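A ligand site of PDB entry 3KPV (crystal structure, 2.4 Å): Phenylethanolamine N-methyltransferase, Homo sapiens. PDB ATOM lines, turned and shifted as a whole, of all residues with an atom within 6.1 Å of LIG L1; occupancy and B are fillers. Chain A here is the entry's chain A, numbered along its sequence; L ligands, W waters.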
ATOM      1  N   TYR A  35      19.264  17.469  24.872  1.00  0.00           N
ATOM      2  CA  TYR A  35      20.135  16.307  24.851  1.00  0.00           C
ATOM      3  C   TYR A  35      19.933  15.455  23.590  1.00  0.00           C
ATOM      4  O   TYR A  35      20.908  15.017  22.979  1.00  0.00           O
ATOM      5  CB  TYR A  35      19.923  15.453  26.090  1.00  0.00           C
ATOM      6  CG  TYR A  35      20.710  14.153  26.082  1.00  0.00           C
ATOM      7  CD1 TYR A  35      22.036  14.121  26.469  1.00  0.00           C
ATOM      8  CD2 TYR A  35      20.097  12.960  25.685  1.00  0.00           C
ATOM      9  CE1 TYR A  35      22.753  12.919  26.466  1.00  0.00           C
ATOM     10  CE2 TYR A  35      20.805  11.766  25.674  1.00  0.00           C
ATOM     11  CZ  TYR A  35      22.127  11.754  26.071  1.00  0.00           C
ATOM     12  OH  TYR A  35      22.827  10.567  26.074  1.00  0.00           O
ATOM     13  N   ASN A  39      22.763  15.096  20.472  1.00  0.00           N
ATOM     14  CA  ASN A  39      23.353  13.767  20.311  1.00  0.00           C
ATOM     15  C   ASN A  39      22.679  12.857  19.296  1.00  0.00           C
ATOM     16  O   ASN A  39      23.317  11.949  18.746  1.00  0.00           O
ATOM     17  CB  ASN A  39      23.443  13.070  21.672  1.00  0.00           C
ATOM     18  CG  ASN A  39      24.449  13.721  22.581  1.00  0.00           C
ATOM     19  OD1 ASN A  39      25.650  13.642  22.359  1.00  0.00           O
ATOM     20  ND2 ASN A  39      23.971  14.389  23.625  1.00  0.00           N
ATOM     21  N   TYR A  40      21.393  13.077  19.051  1.00  0.00           N
ATOM     22  CA  TYR A  40      20.647  12.158  18.199  1.00  0.00           C
ATOM     23  C   TYR A  40      19.996  12.827  17.009  1.00  0.00           C
ATOM     24  O   TYR A  40      19.215  12.204  16.283  1.00  0.00           O
ATOM     25  CB  TYR A  40      19.655  11.359  19.042  1.00  0.00           C
ATOM     26  CG  TYR A  40      20.405  10.515  20.038  1.00  0.00           C
ATOM     27  CD1 TYR A  40      20.581  10.932  21.353  1.00  0.00           C
ATOM     28  CD2 TYR A  40      21.005   9.325  19.645  1.00  0.00           C
ATOM     29  CE1 TYR A  40      21.298  10.178  22.252  1.00  0.00           C
ATOM     30  CE2 TYR A  40      21.722   8.561  20.534  1.00  0.00           C
ATOM     31  CZ  TYR A  40      21.865   8.985  21.840  1.00  0.00           C
ATOM     32  OH  TYR A  40      22.595   8.215  22.724  1.00  0.00           O
ATOM     33  N   ARG A  44      25.639  14.236  14.670  1.00  0.00           N
ATOM     34  CA  ARG A  44      25.891  13.016  15.454  1.00  0.00           C
ATOM     35  C   ARG A  44      24.853  11.938  15.202  1.00  0.00           C
ATOM     36  O   ARG A  44      25.147  10.753  15.325  1.00  0.00           O
ATOM     37  CB  ARG A  44      25.947  13.334  16.944  1.00  0.00           C
ATOM     38  CG  ARG A  44      27.121  14.217  17.297  1.00  0.00           C
ATOM     39  CD  ARG A  44      27.709  13.821  18.606  1.00  0.00           C
ATOM     40  NE  ARG A  44      28.977  14.488  18.862  1.00  0.00           N
ATOM     41  CZ  ARG A  44      29.540  14.528  20.064  1.00  0.00           C
ATOM     42  NH1 ARG A  44      28.922  13.950  21.086  1.00  0.00           N
ATOM     43  NH2 ARG A  44      30.700  15.160  20.239  1.00  0.00           N
ATOM     44  N   LYS A  57      27.510   2.338  16.959  1.00  0.00           N
ATOM     45  CA  LYS A  57      26.830   1.885  18.177  1.00  0.00           C
ATOM     46  C   LYS A  57      25.802   0.803  17.867  1.00  0.00           C
ATOM     47  O   LYS A  57      25.780  -0.249  18.514  1.00  0.00           O
ATOM     48  CB  LYS A  57      26.166   3.060  18.887  1.00  0.00           C
ATOM     49  CG  LYS A  57      27.160   4.117  19.347  1.00  0.00           C
ATOM     50  CD  LYS A  57      26.608   4.968  20.472  1.00  0.00           C
ATOM     51  CE  LYS A  57      25.354   5.709  20.050  1.00  0.00           C
ATOM     52  NZ  LYS A  57      24.775   6.515  21.150  1.00  0.00           N
ATOM     53  N   TYR A  85      17.066   3.693  21.236  1.00  0.00           N
ATOM     54  CA  TYR A  85      17.871   3.034  20.192  1.00  0.00           C
ATOM     55  C   TYR A  85      18.648   1.862  20.752  1.00  0.00           C
ATOM     56  O   TYR A  85      18.894   0.878  20.053  1.00  0.00           O
ATOM     57  CB  TYR A  85      18.865   4.020  19.563  1.00  0.00           C
ATOM     58  CG  TYR A  85      19.998   4.342  20.499  1.00  0.00           C
ATOM     59  CD1 TYR A  85      21.202   3.659  20.441  1.00  0.00           C
ATOM     60  CD2 TYR A  85      19.847   5.322  21.477  1.00  0.00           C
ATOM     61  CE1 TYR A  85      22.251   3.945  21.319  1.00  0.00           C
ATOM     62  CE2 TYR A  85      20.876   5.620  22.352  1.00  0.00           C
ATOM     63  CZ  TYR A  85      22.076   4.925  22.275  1.00  0.00           C
ATOM     64  OH  TYR A  85      23.079   5.234  23.158  1.00  0.00           O
ATOM     65  N   ALA A 181      23.892   2.726  28.515  1.00  0.00           N
ATOM     66  CA  ALA A 181      24.627   3.564  27.591  1.00  0.00           C
ATOM     67  C   ALA A 181      24.749   4.984  28.112  1.00  0.00           C
ATOM     68  O   ALA A 181      23.748   5.666  28.303  1.00  0.00           O
ATOM     69  CB  ALA A 181      23.961   3.541  26.201  1.00  0.00           C
ATOM     70  N   PHE A 182      25.993   5.398  28.338  1.00  0.00           N
ATOM     71  CA  PHE A 182      26.306   6.772  28.706  1.00  0.00           C
ATOM     72  C   PHE A 182      25.689   7.172  30.035  1.00  0.00           C
ATOM     73  O   PHE A 182      25.294   8.325  30.214  1.00  0.00           O
ATOM     74  CB  PHE A 182      25.882   7.753  27.592  1.00  0.00           C
ATOM     75  CG  PHE A 182      26.506   7.457  26.255  1.00  0.00           C
ATOM     76  CD1 PHE A 182      25.791   6.769  25.279  1.00  0.00           C
ATOM     77  CD2 PHE A 182      27.806   7.859  25.974  1.00  0.00           C
ATOM     78  CE1 PHE A 182      26.372   6.491  24.046  1.00  0.00           C
ATOM     79  CE2 PHE A 182      28.387   7.591  24.751  1.00  0.00           C
ATOM     80  CZ  PHE A 182      27.664   6.899  23.780  1.00  0.00           C
ATOM     81  N   GLU A 185      29.629   6.668  33.802  1.00  0.00           N
ATOM     82  CA  GLU A 185      30.672   7.689  33.740  1.00  0.00           C
ATOM     83  C   GLU A 185      30.051   9.079  33.729  1.00  0.00           C
ATOM     84  O   GLU A 185      30.659  10.045  34.183  1.00  0.00           O
ATOM     85  CB  GLU A 185      31.591   7.490  32.526  1.00  0.00           C
ATOM     86  CG  GLU A 185      31.012   7.883  31.158  1.00  0.00           C
ATOM     87  CD  GLU A 185      30.044   6.845  30.552  1.00  0.00           C
ATOM     88  OE1 GLU A 185      29.835   5.763  31.162  1.00  0.00           O
ATOM     89  OE2 GLU A 185      29.504   7.119  29.459  1.00  0.00           O
ATOM     90  N   ALA A 186      28.828   9.179  33.200  1.00  0.00           N
ATOM     91  CA  ALA A 186      28.140  10.455  33.091  1.00  0.00           C
ATOM     92  C   ALA A 186      27.527  10.922  34.421  1.00  0.00           C
ATOM     93  O   ALA A 186      27.091  12.061  34.531  1.00  0.00           O
ATOM     94  CB  ALA A 186      27.054  10.362  32.014  1.00  0.00           C
ATOM     95  N   ALA A 216      31.036   7.050  27.113  1.00  0.00           N
ATOM     96  CA  ALA A 216      31.968   8.055  26.597  1.00  0.00           C
ATOM     97  C   ALA A 216      33.397   7.845  27.086  1.00  0.00           C
ATOM     98  O   ALA A 216      33.635   7.504  28.242  1.00  0.00           O
ATOM     99  CB  ALA A 216      31.484   9.444  26.977  1.00  0.00           C
ATOM    100  N   GLU A 219      35.891  11.785  28.445  1.00  0.00           N
ATOM    101  CA  GLU A 219      35.007  12.941  28.461  1.00  0.00           C
ATOM    102  C   GLU A 219      34.983  13.501  29.885  1.00  0.00           C
ATOM    103  O   GLU A 219      35.046  12.747  30.847  1.00  0.00           O
ATOM    104  CB  GLU A 219      33.599  12.528  28.031  1.00  0.00           C
ATOM    105  CG  GLU A 219      32.567  13.629  28.185  1.00  0.00           C
ATOM    106  CD  GLU A 219      31.280  13.312  27.436  1.00  0.00           C
ATOM    107  OE1 GLU A 219      31.353  13.140  26.198  1.00  0.00           O
ATOM    108  OE2 GLU A 219      30.210  13.230  28.075  1.00  0.00           O
ATOM    109  N   TRP A 221      32.995  16.698  30.421  1.00  0.00           N
ATOM    110  CA  TRP A 221      31.741  17.444  30.514  1.00  0.00           C
ATOM    111  C   TRP A 221      30.888  17.237  29.276  1.00  0.00           C
ATOM    112  O   TRP A 221      31.398  16.871  28.229  1.00  0.00           O
ATOM    113  CB  TRP A 221      32.022  18.946  30.701  1.00  0.00           C
ATOM    114  CG  TRP A 221      32.772  19.560  29.562  1.00  0.00           C
ATOM    115  CD1 TRP A 221      34.133  19.640  29.423  1.00  0.00           C
ATOM    116  CD2 TRP A 221      32.211  20.181  28.406  1.00  0.00           C
ATOM    117  NE1 TRP A 221      34.450  20.274  28.248  1.00  0.00           N
ATOM    118  CE2 TRP A 221      33.286  20.606  27.604  1.00  0.00           C
ATOM    119  CE3 TRP A 221      30.904  20.402  27.950  1.00  0.00           C
ATOM    120  CZ2 TRP A 221      33.089  21.258  26.374  1.00  0.00           C
ATOM    121  CZ3 TRP A 221      30.719  21.047  26.737  1.00  0.00           C
ATOM    122  CH2 TRP A 221      31.797  21.473  25.967  1.00  0.00           C
ATOM    123  N   TYR A 222      29.592  17.452  29.420  1.00  0.00           N
ATOM    124  CA  TYR A 222      28.705  17.545  28.262  1.00  0.00           C
ATOM    125  C   TYR A 222      27.519  18.429  28.625  1.00  0.00           C
ATOM    126  O   TYR A 222      27.238  18.618  29.807  1.00  0.00           O
ATOM    127  CB  TYR A 222      28.268  16.165  27.740  1.00  0.00           C
ATOM    128  CG  TYR A 222      27.221  15.464  28.570  1.00  0.00           C
ATOM    129  CD1 TYR A 222      25.883  15.501  28.187  1.00  0.00           C
ATOM    130  CD2 TYR A 222      27.555  14.748  29.717  1.00  0.00           C
ATOM    131  CE1 TYR A 222      24.898  14.855  28.927  1.00  0.00           C
ATOM    132  CE2 TYR A 222      26.574  14.104  30.466  1.00  0.00           C
ATOM    133  CZ  TYR A 222      25.252  14.161  30.063  1.00  0.00           C
ATOM    134  OH  TYR A 222      24.263  13.526  30.781  1.00  0.00           O
ATOM    135  N   VAL A 231      31.713  14.944  34.046  1.00  0.00           N
ATOM    136  CA  VAL A 231      31.887  13.554  33.679  1.00  0.00           C
ATOM    137  C   VAL A 231      33.250  13.113  34.176  1.00  0.00           C
ATOM    138  O   VAL A 231      34.203  13.892  34.134  1.00  0.00           O
ATOM    139  CB  VAL A 231      31.858  13.384  32.144  1.00  0.00           C
ATOM    140  CG1 VAL A 231      31.996  11.900  31.762  1.00  0.00           C
ATOM    141  CG2 VAL A 231      30.599  14.011  31.553  1.00  0.00           C
ATOM    142  N   MET A 258      36.349   9.328  17.986  1.00  0.00           N
ATOM    143  CA  MET A 258      35.457  10.386  17.503  1.00  0.00           C
ATOM    144  C   MET A 258      36.120  11.286  16.447  1.00  0.00           C
ATOM    145  O   MET A 258      37.040  12.030  16.744  1.00  0.00           O
ATOM    146  CB  MET A 258      34.946  11.219  18.691  1.00  0.00           C
ATOM    147  CG  MET A 258      33.834  12.211  18.335  1.00  0.00           C
ATOM    148  SD  MET A 258      32.216  11.448  18.069  1.00  0.00           S
ATOM    149  CE  MET A 258      32.183  10.243  19.369  1.00  0.00           C
ATOM    150  N   ASP A 267      30.140  18.725  23.918  1.00  0.00           N
ATOM    151  CA  ASP A 267      30.925  18.008  24.915  1.00  0.00           C
ATOM    152  C   ASP A 267      32.397  17.989  24.511  1.00  0.00           C
ATOM    153  O   ASP A 267      32.808  18.697  23.593  1.00  0.00           O
ATOM    154  CB  ASP A 267      30.422  16.569  25.100  1.00  0.00           C
ATOM    155  CG  ASP A 267      30.416  15.777  23.801  1.00  0.00           C
ATOM    156  OD1 ASP A 267      31.434  15.786  23.062  1.00  0.00           O
ATOM    157  OD2 ASP A 267      29.384  15.135  23.505  1.00  0.00           O
ATOM    158  N   VAL A 269      33.961  14.708  24.314  1.00  0.00           N
ATOM    159  CA  VAL A 269      34.168  13.277  24.169  1.00  0.00           C
ATOM    160  C   VAL A 269      35.333  13.035  23.205  1.00  0.00           C
ATOM    161  O   VAL A 269      35.539  13.804  22.257  1.00  0.00           O
ATOM    162  CB  VAL A 269      32.884  12.596  23.626  1.00  0.00           C
ATOM    163  CG1 VAL A 269      32.578  13.086  22.214  1.00  0.00           C
ATOM    164  CG2 VAL A 269      33.013  11.075  23.649  1.00  0.00           C
ATOM    165  N   VAL A 272      34.124   6.454  21.896  1.00  0.00           N
ATOM    166  CA  VAL A 272      33.041   5.704  22.507  1.00  0.00           C
ATOM    167  C   VAL A 272      33.485   4.255  22.669  1.00  0.00           C
ATOM    168  O   VAL A 272      34.022   3.663  21.743  1.00  0.00           O
ATOM    169  CB  VAL A 272      31.766   5.744  21.624  1.00  0.00           C
ATOM    170  CG1 VAL A 272      30.686   4.853  22.199  1.00  0.00           C
ATOM    171  CG2 VAL A 272      31.273   7.169  21.464  1.00  0.00           C
HETATM  172  N1  LIG L   1      26.034  10.260  23.390  1.00  0.00           N
HETATM  173  C1  LIG L   1      25.131  10.124  24.405  1.00  0.00           C
HETATM  174  N2  LIG L   1      25.654  10.713  25.533  1.00  0.00           N
HETATM  175  C2  LIG L   1      26.855  11.216  25.204  1.00  0.00           C
HETATM  176  C3  LIG L   1      27.814  11.909  25.963  1.00  0.00           C
HETATM  177  N3  LIG L   1      27.590  12.177  27.384  1.00  0.00           N
HETATM  178  N4  LIG L   1      28.964  12.302  25.375  1.00  0.00           N
HETATM  179  C4  LIG L   1      29.191  12.019  24.043  1.00  0.00           C
HETATM  180  N5  LIG L   1      28.261  11.328  23.293  1.00  0.00           N
HETATM  181  C5  LIG L   1      27.095  10.938  23.876  1.00  0.00           C
HETATM  182  N1  LG2 L   2      20.991   5.873  27.849  1.00  0.00           N
HETATM  183  C1  LG2 L   2      21.019   7.222  27.289  1.00  0.00           C
HETATM  184  C2  LG2 L   2      21.966   8.045  28.177  1.00  0.00           C
HETATM  185  C3  LG2 L   2      21.200   9.199  28.813  1.00  0.00           C
HETATM  186  S1  LG2 L   2      22.414  10.382  29.467  1.00  0.00           S
HETATM  187  C4  LG2 L   2      21.620   7.140  25.875  1.00  0.00           C
HETATM  188  O1  LG2 L   2      22.163   6.142  25.533  1.00  0.00           O
HETATM  189  O2  LG2 L   2      21.885   8.320  25.182  1.00  0.00           O
HETATM  190  C5  LG2 L   2      22.822   9.945  31.179  1.00  0.00           C
HETATM  191  C6  LG2 L   2      21.548   9.485  31.918  1.00  0.00           C
HETATM  192  O3  LG2 L   2      21.845   9.137  33.303  1.00  0.00           O
HETATM  193  C7  LG2 L   2      20.502  10.595  31.978  1.00  0.00           C
HETATM  194  O4  LG2 L   2      19.271  10.127  31.458  1.00  0.00           O
HETATM  195  C8  LG2 L   2      20.387  10.890  33.447  1.00  0.00           C
HETATM  196  O5  LG2 L   2      19.117  11.382  33.793  1.00  0.00           O
HETATM  197  C9  LG2 L   2      20.652   9.521  34.060  1.00  0.00           C
HETATM  198  N2  LG2 L   2      21.067   9.714  35.435  1.00  0.00           N
HETATM  199  C10 LG2 L   2      21.533  10.992  36.036  1.00  0.00           C
HETATM  200  N3  LG2 L   2      21.901  10.722  37.422  1.00  0.00           N
HETATM  201  C11 LG2 L   2      21.674   9.297  37.684  1.00  0.00           C
HETATM  202  C12 LG2 L   2      21.870   8.457  38.921  1.00  0.00           C
HETATM  203  N4  LG2 L   2      22.395   9.064  40.144  1.00  0.00           N
HETATM  204  N5  LG2 L   2      21.557   7.030  38.890  1.00  0.00           N
HETATM  205  C13 LG2 L   2      21.033   6.403  37.625  1.00  0.00           C
HETATM  206  N6  LG2 L   2      20.829   7.238  36.415  1.00  0.00           N
HETATM  207  C14 LG2 L   2      21.150   8.669  36.442  1.00  0.00           C
HETATM  208  O   HOH W   1      26.696  11.827  20.490  1.00  0.00           O
HETATM  209  O   HOH W   2      27.056  14.861  24.739  1.00  0.00           O
HETATM  210  O   HOH W   3      25.326  11.060  28.427  1.00  0.00           O
HETATM  211  O   HOH W   4      28.574  10.241  20.469  1.00  0.00           O
HETATM  212  O   HOH W   5      26.553   8.989  21.229  1.00  0.00           O
HETATM  213  O   HOH W   6      28.487   9.802  28.914  1.00  0.00           O
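The side-chain carboxylate of Asp 267 lies close to a nitrogen (N4) of LIG L1, 3.4 Å away.
Merely in contact with LIG L1: Asn 39 (3.4 Å), Tyr 40 (3.6 Å), Phe 182 (3.4 Å), Tyr 222 (3.5 Å) and Val 269 (3.8 Å).
Hydrophobic or aromatic side chains within 4 Å of LIG L1: Tyr 35, Phe 182, Tyr 222 and Val 269.
Of the 19 residues printed, 9 come within 4 Å of LIG L1.
The nearest printed residue that does not touch LIG L1 is Ala 216 (4.1 Å).
OD2 of Asp 267 is in salt-bridge range of NH1 of Arg 44, 2.7 Å away.
O of Tyr 35 is in hydrogen-bond range of ND2 of Asn 39.
OH of Tyr 40 lies within hydrogen-bond range of OH of Tyr 85 (3.1 Å).
The side-chain carboxylate of Asp 267 is in hydrogen-bond range of the backbone NH of Val 269, 3.0 Å away.
OH of Tyr 40 is in hydrogen-bond range of NZ of Lys 57, 3.2 Å away.
Water W5 lies within hydrogen-bond range of N1 of LIG L1 (2.6 Å) and NZ of Lys 57 (3.0 Å).
Water W3 lies within hydrogen-bond range of N3 of LIG L1 (2.7 Å), S1 of LG2 L2 (3.2 Å), O of Phe 182 (3.3 Å) and OH of Tyr 35 (3.5 Å).
Water W6 lies within hydrogen-bond range of the side-chain carboxylate of Glu 185 (2.9 Å) and a nitrogen (N3) of LIG L1 (3.0 Å).
Water W1 lies within hydrogen-bond range of OD1 of Asn 39, NH1 of Arg 44 and N5 of LIG L1.
The guanidinium group of Arg 44 is in hydrogen-bond range of a nitrogen (N5) of LIG L1 (3.5 Å).
OH of Tyr 85 is in hydrogen-bond range of O1 of LG2 L2, at 2.7 Å.
The side-chain hydroxyl of Tyr 35 sits at hydrogen-bond distance from an oxygen (O2) of LG2 L2 (2.6 Å).
An oxygen (O2) of LG2 L2 lies within hydrogen-bond range of the side-chain hydroxyl of Tyr 40 (2.6 Å).
O of Ala 181 lies within hydrogen-bond range of N1 of LG2 L2 (2.8 Å).
N2 of LIG L1 lies close to OH of Tyr 35.
OE1 of Glu 219 is in hydrogen-bond range of N4 of LIG L1, 2.7 Å away.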
